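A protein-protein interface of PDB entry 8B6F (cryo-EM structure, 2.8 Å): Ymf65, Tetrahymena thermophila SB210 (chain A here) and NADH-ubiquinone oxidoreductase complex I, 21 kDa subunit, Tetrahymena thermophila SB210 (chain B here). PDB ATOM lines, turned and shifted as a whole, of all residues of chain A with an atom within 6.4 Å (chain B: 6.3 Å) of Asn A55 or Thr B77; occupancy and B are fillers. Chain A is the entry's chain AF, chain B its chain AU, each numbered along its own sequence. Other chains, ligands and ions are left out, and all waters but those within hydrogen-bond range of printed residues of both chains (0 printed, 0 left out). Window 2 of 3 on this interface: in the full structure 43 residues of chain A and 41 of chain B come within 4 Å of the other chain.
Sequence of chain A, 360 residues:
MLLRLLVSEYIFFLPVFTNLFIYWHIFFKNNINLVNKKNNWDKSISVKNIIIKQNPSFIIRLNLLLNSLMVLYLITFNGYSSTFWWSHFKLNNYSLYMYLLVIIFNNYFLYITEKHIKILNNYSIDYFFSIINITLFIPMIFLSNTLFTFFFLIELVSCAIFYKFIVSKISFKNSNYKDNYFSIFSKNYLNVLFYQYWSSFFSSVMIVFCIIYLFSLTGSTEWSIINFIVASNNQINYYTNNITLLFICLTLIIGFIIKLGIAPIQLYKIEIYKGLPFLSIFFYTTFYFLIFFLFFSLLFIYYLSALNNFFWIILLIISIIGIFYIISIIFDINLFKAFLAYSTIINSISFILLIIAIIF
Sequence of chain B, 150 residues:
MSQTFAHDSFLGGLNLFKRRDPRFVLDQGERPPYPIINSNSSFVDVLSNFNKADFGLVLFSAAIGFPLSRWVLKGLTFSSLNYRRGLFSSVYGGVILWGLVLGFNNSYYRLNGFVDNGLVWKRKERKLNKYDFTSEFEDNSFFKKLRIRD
The backbone NH (N) of Asn A55 lies within hydrogen-bond range of the side-chain hydroxyl (OG1) of Thr B77. The side-chain amide oxygen (OE1) of Gln A54 sits close to the backbone carbonyl oxygen (O) of Phe B78 (3.4 Å). The backbone NH of Phe A58 is in hydrogen-bond range of the backbone carbonyl oxygen of Gly B75 (3.4 Å).
The side-chain amide oxygen (OD1) of Asn A55 is in hydrogen-bond range of the backbone NH (N) of Ser A57, 2.7 Å away.
O of Lys A53 touches CD2 of Phe B78, at 3.2 Å. Gln A54 touches Thr B77. O of Gly B75 touches O of Asn A55, at 3.9 Å. CB of Ser A57 touches O of Gly B75, 3.5 Å away. Leu B76 touches Phe A58.
Of the printed residues of chain B, Gln A54 touches Thr B77 and Phe B78. Asn A55 touches just these residues of chain B: Gly B75 and Thr B77. Printed residues of chain B within 4 Å of Phe A58: Gly B75 (3.4 Å) and Leu B76 (3.8 Å). Ile A60 touches none of the printed residues of chain B. Lys B74 touches none of the printed residues of chain A. Of the printed residues of chain A, Leu B76 touches Phe A58. Printed residues of chain A within 4 Å of Thr B77: Gln A54 (3.4 Å) and Asn A55 (3.3 Å). Of the printed residues of chain A, Phe B78 touches Lys A53 and Gln A54. The nearest residue of chain B that does not touch Asn A55 is Leu B76 (5.2 Å). The nearest residue of chain A that does not touch Thr B77 is Lys A53 (4.3 Å).
Of the 8 printed residues of chain B, 4 touch a printed residue of chain A. Among the printed residues, no Asp or Glu carboxylate lies within 4 Å of a Lys or Arg side-chain nitrogen of the other chain.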
ATOM      1  N   LYS A  53      -6.184   8.551  31.702  1.00  0.00           N
ATOM      2  CA  LYS A  53      -5.206   9.214  30.835  1.00  0.00           C
ATOM      3  C   LYS A  53      -5.295   8.523  29.474  1.00  0.00           C
ATOM      4  O   LYS A  53      -4.609   7.530  29.223  1.00  0.00           O
ATOM      5  CB  LYS A  53      -3.799   9.140  31.417  1.00  0.00           C
ATOM      6  CG  LYS A  53      -2.793  10.068  30.749  1.00  0.00           C
ATOM      7  CD  LYS A  53      -3.080  11.528  31.077  1.00  0.00           C
ATOM      8  CE  LYS A  53      -1.993  12.448  30.545  1.00  0.00           C
ATOM      9  NZ  LYS A  53      -1.866  12.370  29.065  1.00  0.00           N
ATOM     10  N   GLN A  54      -6.143   9.058  28.600  1.00  0.00           N
ATOM     11  CA  GLN A  54      -6.399   8.411  27.320  1.00  0.00           C
ATOM     12  C   GLN A  54      -5.225   8.611  26.373  1.00  0.00           C
ATOM     13  O   GLN A  54      -4.735   9.731  26.196  1.00  0.00           O
ATOM     14  CB  GLN A  54      -7.677   8.959  26.688  1.00  0.00           C
ATOM     15  CG  GLN A  54      -8.944   8.585  27.431  1.00  0.00           C
ATOM     16  CD  GLN A  54     -10.201   8.887  26.636  1.00  0.00           C
ATOM     17  OE1 GLN A  54     -11.218   8.211  26.790  1.00  0.00           O
ATOM     18  NE2 GLN A  54     -10.144   9.911  25.789  1.00  0.00           N
ATOM     19  N   ASN A  55      -4.782   7.520  25.761  1.00  0.00           N
ATOM     20  CA  ASN A  55      -3.749   7.606  24.744  1.00  0.00           C
ATOM     21  C   ASN A  55      -4.339   8.203  23.466  1.00  0.00           C
ATOM     22  O   ASN A  55      -5.451   7.841  23.069  1.00  0.00           O
ATOM     23  CB  ASN A  55      -3.168   6.220  24.469  1.00  0.00           C
ATOM     24  CG  ASN A  55      -2.004   6.256  23.505  1.00  0.00           C
ATOM     25  OD1 ASN A  55      -2.119   6.765  22.392  1.00  0.00           O
ATOM     26  ND2 ASN A  55      -0.870   5.715  23.929  1.00  0.00           N
ATOM     27  N   PRO A  56      -3.630   9.119  22.802  1.00  0.00           N
ATOM     28  CA  PRO A  56      -4.168   9.750  21.592  1.00  0.00           C
ATOM     29  C   PRO A  56      -4.015   8.926  20.325  1.00  0.00           C
ATOM     30  O   PRO A  56      -4.200   9.469  19.233  1.00  0.00           O
ATOM     31  CB  PRO A  56      -3.342  11.040  21.498  1.00  0.00           C
ATOM     32  CG  PRO A  56      -2.035  10.668  22.071  1.00  0.00           C
ATOM     33  CD  PRO A  56      -2.315   9.675  23.167  1.00  0.00           C
ATOM     34  N   SER A  57      -3.696   7.637  20.442  1.00  0.00           N
ATOM     35  CA  SER A  57      -3.537   6.803  19.257  1.00  0.00           C
ATOM     36  C   SER A  57      -4.797   6.811  18.401  1.00  0.00           C
ATOM     37  O   SER A  57      -4.718   6.790  17.168  1.00  0.00           O
ATOM     38  CB  SER A  57      -3.181   5.377  19.672  1.00  0.00           C
ATOM     39  OG  SER A  57      -3.018   4.542  18.540  1.00  0.00           O
ATOM     40  N   PHE A  58      -5.971   6.835  19.032  1.00  0.00           N
ATOM     41  CA  PHE A  58      -7.210   6.845  18.262  1.00  0.00           C
ATOM     42  C   PHE A  58      -7.389   8.164  17.518  1.00  0.00           C
ATOM     43  O   PHE A  58      -7.891   8.180  16.389  1.00  0.00           O
ATOM     44  CB  PHE A  58      -8.407   6.558  19.172  1.00  0.00           C
ATOM     45  CG  PHE A  58      -8.694   7.640  20.174  1.00  0.00           C
ATOM     46  CD1 PHE A  58      -7.968   7.728  21.350  1.00  0.00           C
ATOM     47  CD2 PHE A  58      -9.716   8.546  19.953  1.00  0.00           C
ATOM     48  CE1 PHE A  58      -8.244   8.712  22.275  1.00  0.00           C
ATOM     49  CE2 PHE A  58      -9.996   9.532  20.874  1.00  0.00           C
ATOM     50  CZ  PHE A  58      -9.259   9.615  22.036  1.00  0.00           C
ATOM     51  N   ILE A  59      -6.987   9.281  18.128  1.00  0.00           N
ATOM     52  CA  ILE A  59      -7.042  10.563  17.427  1.00  0.00           C
ATOM     53  C   ILE A  59      -6.113  10.549  16.221  1.00  0.00           C
ATOM     54  O   ILE A  59      -6.471  11.022  15.138  1.00  0.00           O
ATOM     55  CB  ILE A  59      -6.699  11.714  18.391  1.00  0.00           C
ATOM     56  CG1 ILE A  59      -7.714  11.783  19.534  1.00  0.00           C
ATOM     57  CG2 ILE A  59      -6.634  13.044  17.642  1.00  0.00           C
ATOM     58  CD1 ILE A  59      -9.114  12.184  19.116  1.00  0.00           C
ATOM     59  N   ILE A  60      -4.900  10.019  16.392  1.00  0.00           N
ATOM     60  CA  ILE A  60      -3.951   9.966  15.283  1.00  0.00           C
ATOM     61  C   ILE A  60      -4.488   9.074  14.172  1.00  0.00           C
ATOM     62  O   ILE A  60      -4.365   9.392  12.984  1.00  0.00           O
ATOM     63  CB  ILE A  60      -2.577   9.485  15.780  1.00  0.00           C
ATOM     64  CG1 ILE A  60      -2.064  10.395  16.894  1.00  0.00           C
ATOM     65  CG2 ILE A  60      -1.579   9.468  14.634  1.00  0.00           C
ATOM     66  CD1 ILE A  60      -0.867   9.838  17.624  1.00  0.00           C
ATOM     67  N   ILE A 117       3.901   7.093  19.548  1.00  0.00           N
ATOM     68  CA  ILE A 117       2.994   7.272  20.678  1.00  0.00           C
ATOM     69  C   ILE A 117       2.682   5.934  21.331  1.00  0.00           C
ATOM     70  O   ILE A 117       2.618   5.828  22.562  1.00  0.00           O
ATOM     71  CB  ILE A 117       1.720   8.011  20.229  1.00  0.00           C
ATOM     72  CG1 ILE A 117       2.062   9.466  19.900  1.00  0.00           C
ATOM     73  CG2 ILE A 117       0.624   7.917  21.290  1.00  0.00           C
ATOM     74  CD1 ILE A 117       2.379  10.317  21.118  1.00  0.00           C
ATOM     75  N   LYS A 118       2.476   4.895  20.526  1.00  0.00           N
ATOM     76  CA  LYS A 118       2.321   3.559  21.092  1.00  0.00           C
ATOM     77  C   LYS A 118       3.547   3.173  21.912  1.00  0.00           C
ATOM     78  O   LYS A 118       3.421   2.528  22.959  1.00  0.00           O
ATOM     79  CB  LYS A 118       2.079   2.548  19.970  1.00  0.00           C
ATOM     80  CG  LYS A 118       0.696   2.644  19.336  1.00  0.00           C
ATOM     81  CD  LYS A 118       0.615   1.808  18.068  1.00  0.00           C
ATOM     82  CE  LYS A 118      -0.691   2.048  17.334  1.00  0.00           C
ATOM     83  NZ  LYS A 118      -0.645   1.488  15.954  1.00  0.00           N
ATOM     84  N   LEU A 120       5.554   5.284  23.590  1.00  0.00           N
ATOM     85  CA  LEU A 120       5.507   6.054  24.823  1.00  0.00           C
ATOM     86  C   LEU A 120       4.614   7.267  24.613  1.00  0.00           C
ATOM     87  O   LEU A 120       4.579   7.849  23.527  1.00  0.00           O
ATOM     88  CB  LEU A 120       6.910   6.489  25.256  1.00  0.00           C
ATOM     89  CG  LEU A 120       6.990   7.282  26.561  1.00  0.00           C
ATOM     90  CD1 LEU A 120       6.479   6.453  27.726  1.00  0.00           C
ATOM     91  CD2 LEU A 120       8.416   7.741  26.811  1.00  0.00           C
ATOM     92  N   ASN A 121       3.907   7.649  25.674  1.00  0.00           N
ATOM     93  CA  ASN A 121       2.898   8.704  25.626  1.00  0.00           C
ATOM     94  C   ASN A 121       3.341   9.865  26.508  1.00  0.00           C
ATOM     95  O   ASN A 121       3.212   9.807  27.735  1.00  0.00           O
ATOM     96  CB  ASN A 121       1.540   8.163  26.063  1.00  0.00           C
ATOM     97  CG  ASN A 121       0.471   9.236  26.104  1.00  0.00           C
ATOM     98  OD1 ASN A 121       0.611  10.292  25.490  1.00  0.00           O
ATOM     99  ND2 ASN A 121      -0.606   8.968  26.832  1.00  0.00           N
ATOM    100  N   TYR A 123       2.349  13.051  25.143  1.00  0.00           N
ATOM    101  CA  TYR A 123       1.633  14.056  24.371  1.00  0.00           C
ATOM    102  C   TYR A 123       0.140  13.899  24.613  1.00  0.00           C
ATOM    103  O   TYR A 123      -0.380  12.779  24.590  1.00  0.00           O
ATOM    104  CB  TYR A 123       1.960  13.920  22.881  1.00  0.00           C
ATOM    105  CG  TYR A 123       3.443  13.814  22.612  1.00  0.00           C
ATOM    106  CD1 TYR A 123       4.094  12.587  22.670  1.00  0.00           C
ATOM    107  CD2 TYR A 123       4.197  14.942  22.320  1.00  0.00           C
ATOM    108  CE1 TYR A 123       5.449  12.486  22.434  1.00  0.00           C
ATOM    109  CE2 TYR A 123       5.553  14.852  22.083  1.00  0.00           C
ATOM    110  CZ  TYR A 123       6.173  13.622  22.142  1.00  0.00           C
ATOM    111  OH  TYR A 123       7.525  13.528  21.907  1.00  0.00           O
ATOM    112  N   ILE A 125      -4.124  14.802  24.106  1.00  0.00           N
ATOM    113  CA  ILE A 125      -5.045  14.754  22.976  1.00  0.00           C
ATOM    114  C   ILE A 125      -5.134  16.111  22.295  1.00  0.00           C
ATOM    115  O   ILE A 125      -5.329  16.190  21.076  1.00  0.00           O
ATOM    116  CB  ILE A 125      -6.425  14.251  23.442  1.00  0.00           C
ATOM    117  CG1 ILE A 125      -6.345  12.757  23.770  1.00  0.00           C
ATOM    118  CG2 ILE A 125      -7.494  14.525  22.385  1.00  0.00           C
ATOM    119  CD1 ILE A 125      -7.592  12.193  24.404  1.00  0.00           C
ATOM    120  N   LEU B  73     -10.781   2.559  16.531  1.00  0.00           N
ATOM    121  CA  LEU B  73     -11.104   2.323  17.934  1.00  0.00           C
ATOM    122  C   LEU B  73     -10.059   1.478  18.648  1.00  0.00           C
ATOM    123  O   LEU B  73      -9.948   1.567  19.874  1.00  0.00           O
ATOM    124  CB  LEU B  73     -12.466   1.639  18.050  1.00  0.00           C
ATOM    125  CG  LEU B  73     -13.576   2.480  18.677  1.00  0.00           C
ATOM    126  CD1 LEU B  73     -13.973   3.617  17.756  1.00  0.00           C
ATOM    127  CD2 LEU B  73     -14.766   1.601  19.007  1.00  0.00           C
ATOM    128  N   LYS B  74      -9.299   0.658  17.922  1.00  0.00           N
ATOM    129  CA  LYS B  74      -8.334  -0.223  18.569  1.00  0.00           C
ATOM    130  C   LYS B  74      -7.225   0.540  19.280  1.00  0.00           C
ATOM    131  O   LYS B  74      -6.489  -0.066  20.066  1.00  0.00           O
ATOM    132  CB  LYS B  74      -7.728  -1.178  17.541  1.00  0.00           C
ATOM    133  CG  LYS B  74      -8.623  -2.357  17.197  1.00  0.00           C
ATOM    134  CD  LYS B  74      -8.060  -3.156  16.035  1.00  0.00           C
ATOM    135  CE  LYS B  74      -9.013  -4.264  15.616  1.00  0.00           C
ATOM    136  NZ  LYS B  74      -8.478  -5.053  14.474  1.00  0.00           N
ATOM    137  N   GLY B  75      -7.082   1.836  19.025  1.00  0.00           N
ATOM    138  CA  GLY B  75      -6.083   2.636  19.705  1.00  0.00           C
ATOM    139  C   GLY B  75      -6.633   3.392  20.897  1.00  0.00           C
ATOM    140  O   GLY B  75      -6.029   4.369  21.350  1.00  0.00           O
ATOM    141  N   LEU B  76      -7.777   2.953  21.413  1.00  0.00           N
ATOM    142  CA  LEU B  76      -8.468   3.637  22.497  1.00  0.00           C
ATOM    143  C   LEU B  76      -8.196   2.941  23.824  1.00  0.00           C
ATOM    144  O   LEU B  76      -8.212   1.710  23.907  1.00  0.00           O
ATOM    145  CB  LEU B  76      -9.973   3.681  22.226  1.00  0.00           C
ATOM    146  CG  LEU B  76     -10.852   4.359  23.277  1.00  0.00           C
ATOM    147  CD1 LEU B  76     -10.428   5.798  23.506  1.00  0.00           C
ATOM    148  CD2 LEU B  76     -12.306   4.295  22.854  1.00  0.00           C
ATOM    149  N   THR B  77      -7.944   3.739  24.861  1.00  0.00           N
ATOM    150  CA  THR B  77      -7.682   3.228  26.198  1.00  0.00           C
ATOM    151  C   THR B  77      -8.355   4.136  27.217  1.00  0.00           C
ATOM    152  O   THR B  77      -8.708   5.279  26.921  1.00  0.00           O
ATOM    153  CB  THR B  77      -6.179   3.136  26.493  1.00  0.00           C
ATOM    154  OG1 THR B  77      -5.597   4.444  26.458  1.00  0.00           O
ATOM    155  CG2 THR B  77      -5.486   2.248  25.471  1.00  0.00           C
ATOM    156  N   PHE B  78      -8.532   3.611  28.429  1.00  0.00           N
ATOM    157  CA  PHE B  78      -9.147   4.364  29.522  1.00  0.00           C
ATOM    158  C   PHE B  78     -10.514   4.907  29.117  1.00  0.00           C
ATOM    159  O   PHE B  78     -10.873   6.043  29.433  1.00  0.00           O
ATOM    160  CB  PHE B  78      -8.237   5.504  29.984  1.00  0.00           C
ATOM    161  CG  PHE B  78      -7.065   5.057  30.803  1.00  0.00           C
ATOM    162  CD1 PHE B  78      -7.174   4.940  32.178  1.00  0.00           C
ATOM    163  CD2 PHE B  78      -5.852   4.774  30.206  1.00  0.00           C
ATOM    164  CE1 PHE B  78      -6.099   4.539  32.939  1.00  0.00           C
ATOM    165  CE2 PHE B  78      -4.770   4.372  30.961  1.00  0.00           C
ATOM    166  CZ  PHE B  78      -4.895   4.255  32.332  1.00  0.00           C
ATOM    167  N   SER B  79     -11.287   4.088  28.414  1.00  0.00           N
ATOM    168  CA  SER B  79     -12.584   4.491  27.892  1.00  0.00           C
ATOM    169  C   SER B  79     -13.671   3.584  28.446  1.00  0.00           C
ATOM    170  O   SER B  79     -13.472   2.374  28.588  1.00  0.00           O
ATOM    171  CB  SER B  79     -12.610   4.441  26.365  1.00  0.00           C
ATOM    172  OG  SER B  79     -12.477   3.110  25.904  1.00  0.00           O
ATOM    173  N   ARG B  84     -16.834   4.367  24.132  1.00  0.00           N
ATOM    174  CA  ARG B  84     -16.316   3.578  23.021  1.00  0.00           C
ATOM    175  C   ARG B  84     -17.372   3.403  21.938  1.00  0.00           C
ATOM    176  O   ARG B  84     -17.081   3.545  20.745  1.00  0.00           O
ATOM    177  CB  ARG B  84     -15.835   2.219  23.525  1.00  0.00           C
ATOM    178  CG  ARG B  84     -15.185   1.357  22.457  1.00  0.00           C
ATOM    179  CD  ARG B  84     -14.752   0.018  23.025  1.00  0.00           C
ATOM    180  NE  ARG B  84     -13.765   0.167  24.088  1.00  0.00           N
ATOM    181  CZ  ARG B  84     -12.454   0.223  23.899  1.00  0.00           C
ATOM    182  NH1 ARG B  84     -11.925   0.152  22.689  1.00  0.00           N
ATOM    183  NH2 ARG B  84     -11.653   0.353  24.952  1.00  0.00           N
